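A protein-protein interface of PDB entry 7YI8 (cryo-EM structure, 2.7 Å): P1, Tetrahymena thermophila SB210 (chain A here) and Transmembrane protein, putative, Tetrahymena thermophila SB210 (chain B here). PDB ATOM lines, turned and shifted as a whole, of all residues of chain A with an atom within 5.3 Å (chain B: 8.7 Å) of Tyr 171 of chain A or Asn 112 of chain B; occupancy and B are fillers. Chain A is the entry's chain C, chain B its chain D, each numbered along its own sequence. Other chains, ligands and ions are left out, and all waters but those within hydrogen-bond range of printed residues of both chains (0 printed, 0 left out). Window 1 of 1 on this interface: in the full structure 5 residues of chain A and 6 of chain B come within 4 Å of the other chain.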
ATOM      1  N   LEU A 164     -19.926 -28.178 -21.826  1.00  0.00           N
ATOM      2  CA  LEU A 164     -21.247 -27.646 -21.516  1.00  0.00           C
ATOM      3  C   LEU A 164     -21.337 -27.130 -20.087  1.00  0.00           C
ATOM      4  O   LEU A 164     -22.039 -26.145 -19.831  1.00  0.00           O
ATOM      5  CB  LEU A 164     -22.312 -28.721 -21.752  1.00  0.00           C
ATOM      6  CG  LEU A 164     -23.781 -28.346 -21.547  1.00  0.00           C
ATOM      7  CD1 LEU A 164     -24.087 -26.964 -22.108  1.00  0.00           C
ATOM      8  CD2 LEU A 164     -24.679 -29.397 -22.178  1.00  0.00           C
ATOM      9  N   GLU A 165     -20.630 -27.768 -19.153  1.00  0.00           N
ATOM     10  CA  GLU A 165     -20.644 -27.358 -17.756  1.00  0.00           C
ATOM     11  C   GLU A 165     -19.733 -26.168 -17.478  1.00  0.00           C
ATOM     12  O   GLU A 165     -19.747 -25.652 -16.356  1.00  0.00           O
ATOM     13  CB  GLU A 165     -20.240 -28.538 -16.866  1.00  0.00           C
ATOM     14  CG  GLU A 165     -20.653 -28.419 -15.407  1.00  0.00           C
ATOM     15  CD  GLU A 165     -20.416 -29.702 -14.633  1.00  0.00           C
ATOM     16  OE1 GLU A 165     -19.968 -30.692 -15.246  1.00  0.00           O
ATOM     17  OE2 GLU A 165     -20.679 -29.719 -13.413  1.00  0.00           O
ATOM     18  N   LEU A 167     -20.103 -23.275 -18.013  1.00  0.00           N
ATOM     19  CA  LEU A 167     -20.957 -22.267 -17.389  1.00  0.00           C
ATOM     20  C   LEU A 167     -21.546 -22.794 -16.083  1.00  0.00           C
ATOM     21  O   LEU A 167     -22.754 -22.750 -15.861  1.00  0.00           O
ATOM     22  CB  LEU A 167     -22.060 -21.847 -18.354  1.00  0.00           C
ATOM     23  CG  LEU A 167     -21.714 -21.264 -19.724  1.00  0.00           C
ATOM     24  CD1 LEU A 167     -21.537 -22.356 -20.766  1.00  0.00           C
ATOM     25  CD2 LEU A 167     -22.794 -20.289 -20.157  1.00  0.00           C
ATOM     26  N   THR A 168     -20.678 -23.299 -15.199  1.00  0.00           N
ATOM     27  CA  THR A 168     -21.153 -23.933 -13.973  1.00  0.00           C
ATOM     28  C   THR A 168     -21.863 -22.941 -13.064  1.00  0.00           C
ATOM     29  O   THR A 168     -22.709 -23.336 -12.254  1.00  0.00           O
ATOM     30  CB  THR A 168     -19.989 -24.594 -13.231  1.00  0.00           C
ATOM     31  OG1 THR A 168     -20.496 -25.353 -12.125  1.00  0.00           O
ATOM     32  CG2 THR A 168     -19.016 -23.545 -12.714  1.00  0.00           C
ATOM     33  N   HIS A 169     -21.534 -21.654 -13.179  1.00  0.00           N
ATOM     34  CA  HIS A 169     -22.253 -20.607 -12.477  1.00  0.00           C
ATOM     35  C   HIS A 169     -22.935 -19.618 -13.405  1.00  0.00           C
ATOM     36  O   HIS A 169     -23.864 -18.937 -12.967  1.00  0.00           O
ATOM     37  CB  HIS A 169     -21.311 -19.828 -11.545  1.00  0.00           C
ATOM     38  CG  HIS A 169     -20.977 -20.547 -10.276  1.00  0.00           C
ATOM     39  ND1 HIS A 169     -19.876 -21.367 -10.153  1.00  0.00           N
ATOM     40  CD2 HIS A 169     -21.596 -20.564  -9.072  1.00  0.00           C
ATOM     41  CE1 HIS A 169     -19.833 -21.861  -8.928  1.00  0.00           C
ATOM     42  NE2 HIS A 169     -20.865 -21.389  -8.251  1.00  0.00           N
ATOM     43  N   LEU A 170     -22.525 -19.538 -14.673  1.00  0.00           N
ATOM     44  CA  LEU A 170     -23.149 -18.601 -15.598  1.00  0.00           C
ATOM     45  C   LEU A 170     -24.610 -18.940 -15.852  1.00  0.00           C
ATOM     46  O   LEU A 170     -25.356 -18.088 -16.350  1.00  0.00           O
ATOM     47  CB  LEU A 170     -22.375 -18.584 -16.917  1.00  0.00           C
ATOM     48  CG  LEU A 170     -20.948 -18.039 -16.840  1.00  0.00           C
ATOM     49  CD1 LEU A 170     -20.228 -18.199 -18.169  1.00  0.00           C
ATOM     50  CD2 LEU A 170     -20.960 -16.586 -16.406  1.00  0.00           C
ATOM     51  N   TYR A 171     -25.033 -20.159 -15.504  1.00  0.00           N
ATOM     52  CA  TYR A 171     -26.414 -20.573 -15.726  1.00  0.00           C
ATOM     53  C   TYR A 171     -27.390 -19.622 -15.046  1.00  0.00           C
ATOM     54  O   TYR A 171     -28.332 -19.127 -15.674  1.00  0.00           O
ATOM     55  CB  TYR A 171     -26.620 -22.002 -15.219  1.00  0.00           C
ATOM     56  CG  TYR A 171     -26.012 -23.072 -16.097  1.00  0.00           C
ATOM     57  CD1 TYR A 171     -25.431 -22.754 -17.317  1.00  0.00           C
ATOM     58  CD2 TYR A 171     -26.020 -24.404 -15.705  1.00  0.00           C
ATOM     59  CE1 TYR A 171     -24.875 -23.734 -18.119  1.00  0.00           C
ATOM     60  CE2 TYR A 171     -25.467 -25.388 -16.502  1.00  0.00           C
ATOM     61  CZ  TYR A 171     -24.897 -25.046 -17.708  1.00  0.00           C
ATOM     62  OH  TYR A 171     -24.342 -26.018 -18.507  1.00  0.00           O
ATOM     63  N   ASN A 172     -27.182 -19.350 -13.757  1.00  0.00           N
ATOM     64  CA  ASN A 172     -28.047 -18.409 -13.060  1.00  0.00           C
ATOM     65  C   ASN A 172     -27.632 -16.957 -13.259  1.00  0.00           C
ATOM     66  O   ASN A 172     -28.461 -16.063 -13.066  1.00  0.00           O
ATOM     67  CB  ASN A 172     -28.126 -18.752 -11.564  1.00  0.00           C
ATOM     68  CG  ASN A 172     -26.783 -18.675 -10.857  1.00  0.00           C
ATOM     69  OD1 ASN A 172     -25.824 -18.108 -11.368  1.00  0.00           O
ATOM     70  ND2 ASN A 172     -26.717 -19.254  -9.664  1.00  0.00           N
ATOM     71  N   LEU A 173     -26.384 -16.694 -13.662  1.00  0.00           N
ATOM     72  CA  LEU A 173     -26.034 -15.338 -14.077  1.00  0.00           C
ATOM     73  C   LEU A 173     -26.815 -14.909 -15.311  1.00  0.00           C
ATOM     74  O   LEU A 173     -27.040 -13.710 -15.508  1.00  0.00           O
ATOM     75  CB  LEU A 173     -24.530 -15.205 -14.331  1.00  0.00           C
ATOM     76  CG  LEU A 173     -23.578 -14.943 -13.158  1.00  0.00           C
ATOM     77  CD1 LEU A 173     -23.895 -13.587 -12.543  1.00  0.00           C
ATOM     78  CD2 LEU A 173     -23.620 -16.015 -12.093  1.00  0.00           C
ATOM     79  N   LYS A 174     -27.252 -15.866 -16.137  1.00  0.00           N
ATOM     80  CA  LYS A 174     -28.071 -15.524 -17.297  1.00  0.00           C
ATOM     81  C   LYS A 174     -29.342 -14.784 -16.893  1.00  0.00           C
ATOM     82  O   LYS A 174     -29.883 -14.004 -17.684  1.00  0.00           O
ATOM     83  CB  LYS A 174     -28.421 -16.785 -18.089  1.00  0.00           C
ATOM     84  CG  LYS A 174     -27.231 -17.472 -18.743  1.00  0.00           C
ATOM     85  CD  LYS A 174     -26.661 -16.646 -19.883  1.00  0.00           C
ATOM     86  CE  LYS A 174     -27.542 -16.727 -21.116  1.00  0.00           C
ATOM     87  NZ  LYS A 174     -26.954 -15.997 -22.272  1.00  0.00           N
ATOM     88  N   ALA A 175     -29.833 -15.015 -15.673  1.00  0.00           N
ATOM     89  CA  ALA A 175     -30.963 -14.267 -15.136  1.00  0.00           C
ATOM     90  C   ALA A 175     -30.550 -13.202 -14.129  1.00  0.00           C
ATOM     91  O   ALA A 175     -31.296 -12.235 -13.928  1.00  0.00           O
ATOM     92  CB  ALA A 175     -31.969 -15.218 -14.479  1.00  0.00           C
ATOM     93  N   GLN B  77     -24.901 -36.131 -19.710  1.00  0.00           N
ATOM     94  CA  GLN B  77     -25.127 -34.872 -20.416  1.00  0.00           C
ATOM     95  C   GLN B  77     -24.814 -35.122 -21.887  1.00  0.00           C
ATOM     96  O   GLN B  77     -23.699 -34.873 -22.347  1.00  0.00           O
ATOM     97  CB  GLN B  77     -24.268 -33.749 -19.837  1.00  0.00           C
ATOM     98  CG  GLN B  77     -24.170 -33.757 -18.323  1.00  0.00           C
ATOM     99  CD  GLN B  77     -23.507 -32.510 -17.772  1.00  0.00           C
ATOM    100  OE1 GLN B  77     -22.722 -31.855 -18.457  1.00  0.00           O
ATOM    101  NE2 GLN B  77     -23.819 -32.174 -16.525  1.00  0.00           N
ATOM    102  N   TRP B  79     -26.601 -34.908 -26.015  1.00  0.00           N
ATOM    103  CA  TRP B  79     -27.649 -34.352 -26.870  1.00  0.00           C
ATOM    104  C   TRP B  79     -28.032 -35.416 -27.892  1.00  0.00           C
ATOM    105  O   TRP B  79     -27.436 -35.523 -28.964  1.00  0.00           O
ATOM    106  CB  TRP B  79     -27.189 -33.062 -27.537  1.00  0.00           C
ATOM    107  CG  TRP B  79     -28.315 -32.255 -28.108  1.00  0.00           C
ATOM    108  CD1 TRP B  79     -28.623 -32.097 -29.426  1.00  0.00           C
ATOM    109  CD2 TRP B  79     -29.291 -31.502 -27.375  1.00  0.00           C
ATOM    110  NE1 TRP B  79     -29.726 -31.290 -29.561  1.00  0.00           N
ATOM    111  CE2 TRP B  79     -30.155 -30.912 -28.317  1.00  0.00           C
ATOM    112  CE3 TRP B  79     -29.515 -31.269 -26.015  1.00  0.00           C
ATOM    113  CZ2 TRP B  79     -31.225 -30.104 -27.943  1.00  0.00           C
ATOM    114  CZ3 TRP B  79     -30.579 -30.469 -25.647  1.00  0.00           C
ATOM    115  CH2 TRP B  79     -31.419 -29.895 -26.606  1.00  0.00           C
ATOM    116  N   ASN B  83     -33.495 -35.401 -28.895  1.00  0.00           N
ATOM    117  CA  ASN B  83     -33.571 -34.031 -28.396  1.00  0.00           C
ATOM    118  C   ASN B  83     -33.540 -33.029 -29.542  1.00  0.00           C
ATOM    119  O   ASN B  83     -34.219 -31.996 -29.493  1.00  0.00           O
ATOM    120  CB  ASN B  83     -32.426 -33.757 -27.422  1.00  0.00           C
ATOM    121  CG  ASN B  83     -32.443 -34.679 -26.223  1.00  0.00           C
ATOM    122  OD1 ASN B  83     -31.577 -35.539 -26.076  1.00  0.00           O
ATOM    123  ND2 ASN B  83     -33.429 -34.500 -25.354  1.00  0.00           N
ATOM    124  N   TRP B  99     -38.154 -19.845 -22.731  1.00  0.00           N
ATOM    125  CA  TRP B  99     -37.953 -21.286 -22.663  1.00  0.00           C
ATOM    126  C   TRP B  99     -38.550 -21.909 -21.403  1.00  0.00           C
ATOM    127  O   TRP B  99     -37.916 -22.756 -20.769  1.00  0.00           O
ATOM    128  CB  TRP B  99     -36.465 -21.619 -22.757  1.00  0.00           C
ATOM    129  CG  TRP B  99     -35.729 -20.825 -23.788  1.00  0.00           C
ATOM    130  CD1 TRP B  99     -35.136 -19.607 -23.620  1.00  0.00           C
ATOM    131  CD2 TRP B  99     -35.500 -21.197 -25.153  1.00  0.00           C
ATOM    132  NE1 TRP B  99     -34.557 -19.196 -24.795  1.00  0.00           N
ATOM    133  CE2 TRP B  99     -34.766 -20.155 -25.752  1.00  0.00           C
ATOM    134  CE3 TRP B  99     -35.848 -22.307 -25.926  1.00  0.00           C
ATOM    135  CZ2 TRP B  99     -34.372 -20.192 -27.087  1.00  0.00           C
ATOM    136  CZ3 TRP B  99     -35.456 -22.341 -27.251  1.00  0.00           C
ATOM    137  CH2 TRP B  99     -34.727 -21.291 -27.817  1.00  0.00           C
ATOM    138  N   ILE B 102     -41.440 -24.643 -23.307  1.00  0.00           N
ATOM    139  CA  ILE B 102     -40.712 -25.678 -24.028  1.00  0.00           C
ATOM    140  C   ILE B 102     -40.164 -26.729 -23.071  1.00  0.00           C
ATOM    141  O   ILE B 102     -39.959 -27.881 -23.471  1.00  0.00           O
ATOM    142  CB  ILE B 102     -39.587 -25.056 -24.879  1.00  0.00           C
ATOM    143  CG1 ILE B 102     -39.125 -26.041 -25.955  1.00  0.00           C
ATOM    144  CG2 ILE B 102     -38.414 -24.629 -24.008  1.00  0.00           C
ATOM    145  CD1 ILE B 102     -40.174 -26.335 -26.998  1.00  0.00           C
ATOM    146  N   ASN B 103     -39.926 -26.363 -21.814  1.00  0.00           N
ATOM    147  CA  ASN B 103     -39.512 -27.307 -20.787  1.00  0.00           C
ATOM    148  C   ASN B 103     -40.658 -27.726 -19.876  1.00  0.00           C
ATOM    149  O   ASN B 103     -40.424 -28.446 -18.900  1.00  0.00           O
ATOM    150  CB  ASN B 103     -38.374 -26.714 -19.950  1.00  0.00           C
ATOM    151  CG  ASN B 103     -37.375 -27.763 -19.502  1.00  0.00           C
ATOM    152  OD1 ASN B 103     -37.019 -28.661 -20.265  1.00  0.00           O
ATOM    153  ND2 ASN B 103     -36.917 -27.654 -18.261  1.00  0.00           N
ATOM    154  N   GLU B 106     -41.714 -30.741 -21.877  1.00  0.00           N
ATOM    155  CA  GLU B 106     -40.471 -31.510 -21.829  1.00  0.00           C
ATOM    156  C   GLU B 106     -40.340 -32.435 -23.038  1.00  0.00           C
ATOM    157  O   GLU B 106     -40.135 -33.643 -22.905  1.00  0.00           O
ATOM    158  CB  GLU B 106     -40.362 -32.296 -20.520  1.00  0.00           C
ATOM    159  CG  GLU B 106     -39.667 -31.536 -19.404  1.00  0.00           C
ATOM    160  CD  GLU B 106     -39.278 -32.429 -18.246  1.00  0.00           C
ATOM    161  OE1 GLU B 106     -39.782 -33.569 -18.176  1.00  0.00           O
ATOM    162  OE2 GLU B 106     -38.465 -31.991 -17.405  1.00  0.00           O
ATOM    163  N   SER B 108     -37.833 -32.394 -25.004  1.00  0.00           N
ATOM    164  CA  SER B 108     -36.515 -32.890 -24.622  1.00  0.00           C
ATOM    165  C   SER B 108     -36.567 -33.157 -23.122  1.00  0.00           C
ATOM    166  O   SER B 108     -36.604 -32.225 -22.316  1.00  0.00           O
ATOM    167  CB  SER B 108     -35.431 -31.884 -24.988  1.00  0.00           C
ATOM    168  OG  SER B 108     -35.838 -30.564 -24.672  1.00  0.00           O
ATOM    169  N   GLY B 109     -36.586 -34.435 -22.747  1.00  0.00           N
ATOM    170  CA  GLY B 109     -36.799 -34.823 -21.365  1.00  0.00           C
ATOM    171  C   GLY B 109     -35.767 -34.307 -20.383  1.00  0.00           C
ATOM    172  O   GLY B 109     -34.569 -34.564 -20.539  1.00  0.00           O
ATOM    173  N   LYS B 110     -36.235 -33.587 -19.360  1.00  0.00           N
ATOM    174  CA  LYS B 110     -35.377 -33.057 -18.297  1.00  0.00           C
ATOM    175  C   LYS B 110     -34.222 -32.240 -18.870  1.00  0.00           C
ATOM    176  O   LYS B 110     -33.074 -32.352 -18.436  1.00  0.00           O
ATOM    177  CB  LYS B 110     -34.859 -34.183 -17.399  1.00  0.00           C
ATOM    178  CG  LYS B 110     -35.705 -34.424 -16.160  1.00  0.00           C
ATOM    179  CD  LYS B 110     -37.024 -35.093 -16.512  1.00  0.00           C
ATOM    180  CE  LYS B 110     -37.901 -35.267 -15.286  1.00  0.00           C
ATOM    181  NZ  LYS B 110     -39.303 -35.612 -15.652  1.00  0.00           N
ATOM    182  N   ALA B 111     -34.535 -31.405 -19.853  1.00  0.00           N
ATOM    183  CA  ALA B 111     -33.529 -30.639 -20.572  1.00  0.00           C
ATOM    184  C   ALA B 111     -33.138 -29.382 -19.801  1.00  0.00           C
ATOM    185  O   ALA B 111     -33.814 -28.959 -18.861  1.00  0.00           O
ATOM    186  CB  ALA B 111     -34.038 -30.269 -21.963  1.00  0.00           C
ATOM    187  N   ASN B 112     -32.026 -28.786 -20.220  1.00  0.00           N
ATOM    188  CA  ASN B 112     -31.454 -27.615 -19.569  1.00  0.00           C
ATOM    189  C   ASN B 112     -31.748 -26.376 -20.406  1.00  0.00           C
ATOM    190  O   ASN B 112     -31.478 -26.359 -21.611  1.00  0.00           O
ATOM    191  CB  ASN B 112     -29.948 -27.806 -19.376  1.00  0.00           C
ATOM    192  CG  ASN B 112     -29.281 -26.614 -18.727  1.00  0.00           C
ATOM    193  OD1 ASN B 112     -28.118 -26.323 -18.999  1.00  0.00           O
ATOM    194  ND2 ASN B 112     -30.008 -25.923 -17.856  1.00  0.00           N
ATOM    195  N   ILE B 113     -32.287 -25.338 -19.759  1.00  0.00           N
ATOM    196  CA  ILE B 113     -32.840 -24.192 -20.482  1.00  0.00           C
ATOM    197  C   ILE B 113     -31.764 -23.493 -21.305  1.00  0.00           C
ATOM    198  O   ILE B 113     -31.959 -23.189 -22.490  1.00  0.00           O
ATOM    199  CB  ILE B 113     -33.511 -23.218 -19.497  1.00  0.00           C
ATOM    200  CG1 ILE B 113     -34.693 -23.891 -18.799  1.00  0.00           C
ATOM    201  CG2 ILE B 113     -33.949 -21.952 -20.212  1.00  0.00           C
ATOM    202  CD1 ILE B 113     -35.245 -23.097 -17.636  1.00  0.00           C
ATOM    203  N   VAL B 114     -30.614 -23.218 -20.686  1.00  0.00           N
ATOM    204  CA  VAL B 114     -29.547 -22.533 -21.407  1.00  0.00           C
ATOM    205  C   VAL B 114     -29.025 -23.400 -22.545  1.00  0.00           C
ATOM    206  O   VAL B 114     -28.607 -22.882 -23.585  1.00  0.00           O
ATOM    207  CB  VAL B 114     -28.422 -22.114 -20.445  1.00  0.00           C
ATOM    208  CG1 VAL B 114     -28.943 -21.104 -19.438  1.00  0.00           C
ATOM    209  CG2 VAL B 114     -27.864 -23.319 -19.739  1.00  0.00           C
ATOM    210  N   GLU B 115     -29.061 -24.724 -22.384  1.00  0.00           N
ATOM    211  CA  GLU B 115     -28.689 -25.604 -23.485  1.00  0.00           C
ATOM    212  C   GLU B 115     -29.671 -25.474 -24.645  1.00  0.00           C
ATOM    213  O   GLU B 115     -29.272 -25.534 -25.813  1.00  0.00           O
ATOM    214  CB  GLU B 115     -28.607 -27.047 -22.994  1.00  0.00           C
ATOM    215  CG  GLU B 115     -28.601 -28.084 -24.096  1.00  0.00           C
ATOM    216  CD  GLU B 115     -27.216 -28.345 -24.642  1.00  0.00           C
ATOM    217  OE1 GLU B 115     -26.292 -27.584 -24.298  1.00  0.00           O
ATOM    218  OE2 GLU B 115     -27.048 -29.310 -25.415  1.00  0.00           O
ATOM    219  N   LEU B 116     -30.960 -25.292 -24.346  1.00  0.00           N
ATOM    220  CA  LEU B 116     -31.934 -25.040 -25.406  1.00  0.00           C
ATOM    221  C   LEU B 116     -31.666 -23.714 -26.106  1.00  0.00           C
ATOM    222  O   LEU B 116     -31.683 -23.640 -27.340  1.00  0.00           O
ATOM    223  CB  LEU B 116     -33.359 -25.071 -24.848  1.00  0.00           C
ATOM    224  CG  LEU B 116     -34.088 -26.413 -24.732  1.00  0.00           C
ATOM    225  CD1 LEU B 116     -34.312 -27.002 -26.112  1.00  0.00           C
ATOM    226  CD2 LEU B 116     -33.333 -27.394 -23.870  1.00  0.00           C
ATOM    227  N   GLU B 117     -31.412 -22.652 -25.338  1.00  0.00           N
ATOM    228  CA  GLU B 117     -31.188 -21.356 -25.974  1.00  0.00           C
ATOM    229  C   GLU B 117     -29.819 -21.254 -26.631  1.00  0.00           C
ATOM    230  O   GLU B 117     -29.580 -20.300 -27.378  1.00  0.00           O
ATOM    231  CB  GLU B 117     -31.370 -20.219 -24.966  1.00  0.00           C
ATOM    232  CG  GLU B 117     -30.351 -20.194 -23.848  1.00  0.00           C
ATOM    233  CD  GLU B 117     -30.616 -19.090 -22.843  1.00  0.00           C
ATOM    234  OE1 GLU B 117     -31.613 -18.357 -23.009  1.00  0.00           O
ATOM    235  OE2 GLU B 117     -29.831 -18.961 -21.881  1.00  0.00           O
ATOM    236  N   LEU B 118     -28.922 -22.202 -26.368  1.00  0.00           N
ATOM    237  CA  LEU B 118     -27.620 -22.250 -27.020  1.00  0.00           C
ATOM    238  C   LEU B 118     -27.628 -23.116 -28.274  1.00  0.00           C
ATOM    239  O   LEU B 118     -27.076 -22.717 -29.303  1.00  0.00           O
ATOM    240  CB  LEU B 118     -26.571 -22.766 -26.030  1.00  0.00           C
ATOM    241  CG  LEU B 118     -25.092 -22.677 -26.396  1.00  0.00           C
ATOM    242  CD1 LEU B 118     -24.275 -22.387 -25.152  1.00  0.00           C
ATOM    243  CD2 LEU B 118     -24.628 -23.968 -27.039  1.00  0.00           C
ATOM    244  N   ARG B 119     -28.244 -24.300 -28.209  1.00  0.00           N
ATOM    245  CA  ARG B 119     -28.288 -25.185 -29.367  1.00  0.00           C
ATOM    246  C   ARG B 119     -29.236 -24.680 -30.444  1.00  0.00           C
ATOM    247  O   ARG B 119     -29.140 -25.125 -31.592  1.00  0.00           O
ATOM    248  CB  ARG B 119     -28.696 -26.594 -28.940  1.00  0.00           C
ATOM    249  CG  ARG B 119     -27.747 -27.240 -27.950  1.00  0.00           C
ATOM    250  CD  ARG B 119     -26.944 -28.356 -28.585  1.00  0.00           C
ATOM    251  NE  ARG B 119     -26.054 -28.983 -27.616  1.00  0.00           N
ATOM    252  CZ  ARG B 119     -25.147 -29.901 -27.917  1.00  0.00           C
ATOM    253  NH1 ARG B 119     -24.983 -30.328 -29.158  1.00  0.00           N
ATOM    254  NH2 ARG B 119     -24.387 -30.402 -26.949  1.00  0.00           N
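The guanidinium group (NE) of Arg 119 of chain B lies within salt-bridge range of the side-chain carboxylate (OE2) of Glu 115 of chain B (2.4 Å). O of Leu 164 of chain A is in hydrogen-bond range of OH of Tyr 171 of chain A.
Of the printed residues of chain B, Leu 164 of chain A touches Glu 115. Tyr 171 of chain A touches two residues of chain B. Printed residues of chain B within 4 Å of Lys 174 of chain A: Glu 117. Glu 106 of chain B touches none of the printed residues of chain A. Of chain A, only Tyr 171 comes within 4 Å of Asn 112 of chain B. Printed residues of chain A within 4 Å of Val 114 of chain B: Tyr 171. Of the printed residues of chain A, Glu 115 of chain B touches Leu 164. The nearest printed residue of chain B that does not touch Lys 174 of chain A is Val 114 of chain B (4.1 Å).
Hydrophobic or aromatic side chains of chain A within 4 Å of the printed part of chain B: Leu 164 and Tyr 171. Along chain B the printed residues that touch a printed residue of chain A span positions 112 to 117. Among the printed residues, 4 pairs touch across the chains.
Glu 115 of chain B touches Leu 164 of chain A (OE1 to CD1, 3.2 Å). CZ of Tyr 171 of chain A touches OD1 of Asn 112 of chain B, 3.7 Å away. CG2 of Val 114 of chain B touches CE1 of Tyr 171 of chain A, at 3.4 Å. Glu 117 of chain B touches Lys 174 of chain A (OE2 to CE, 3.3 Å).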
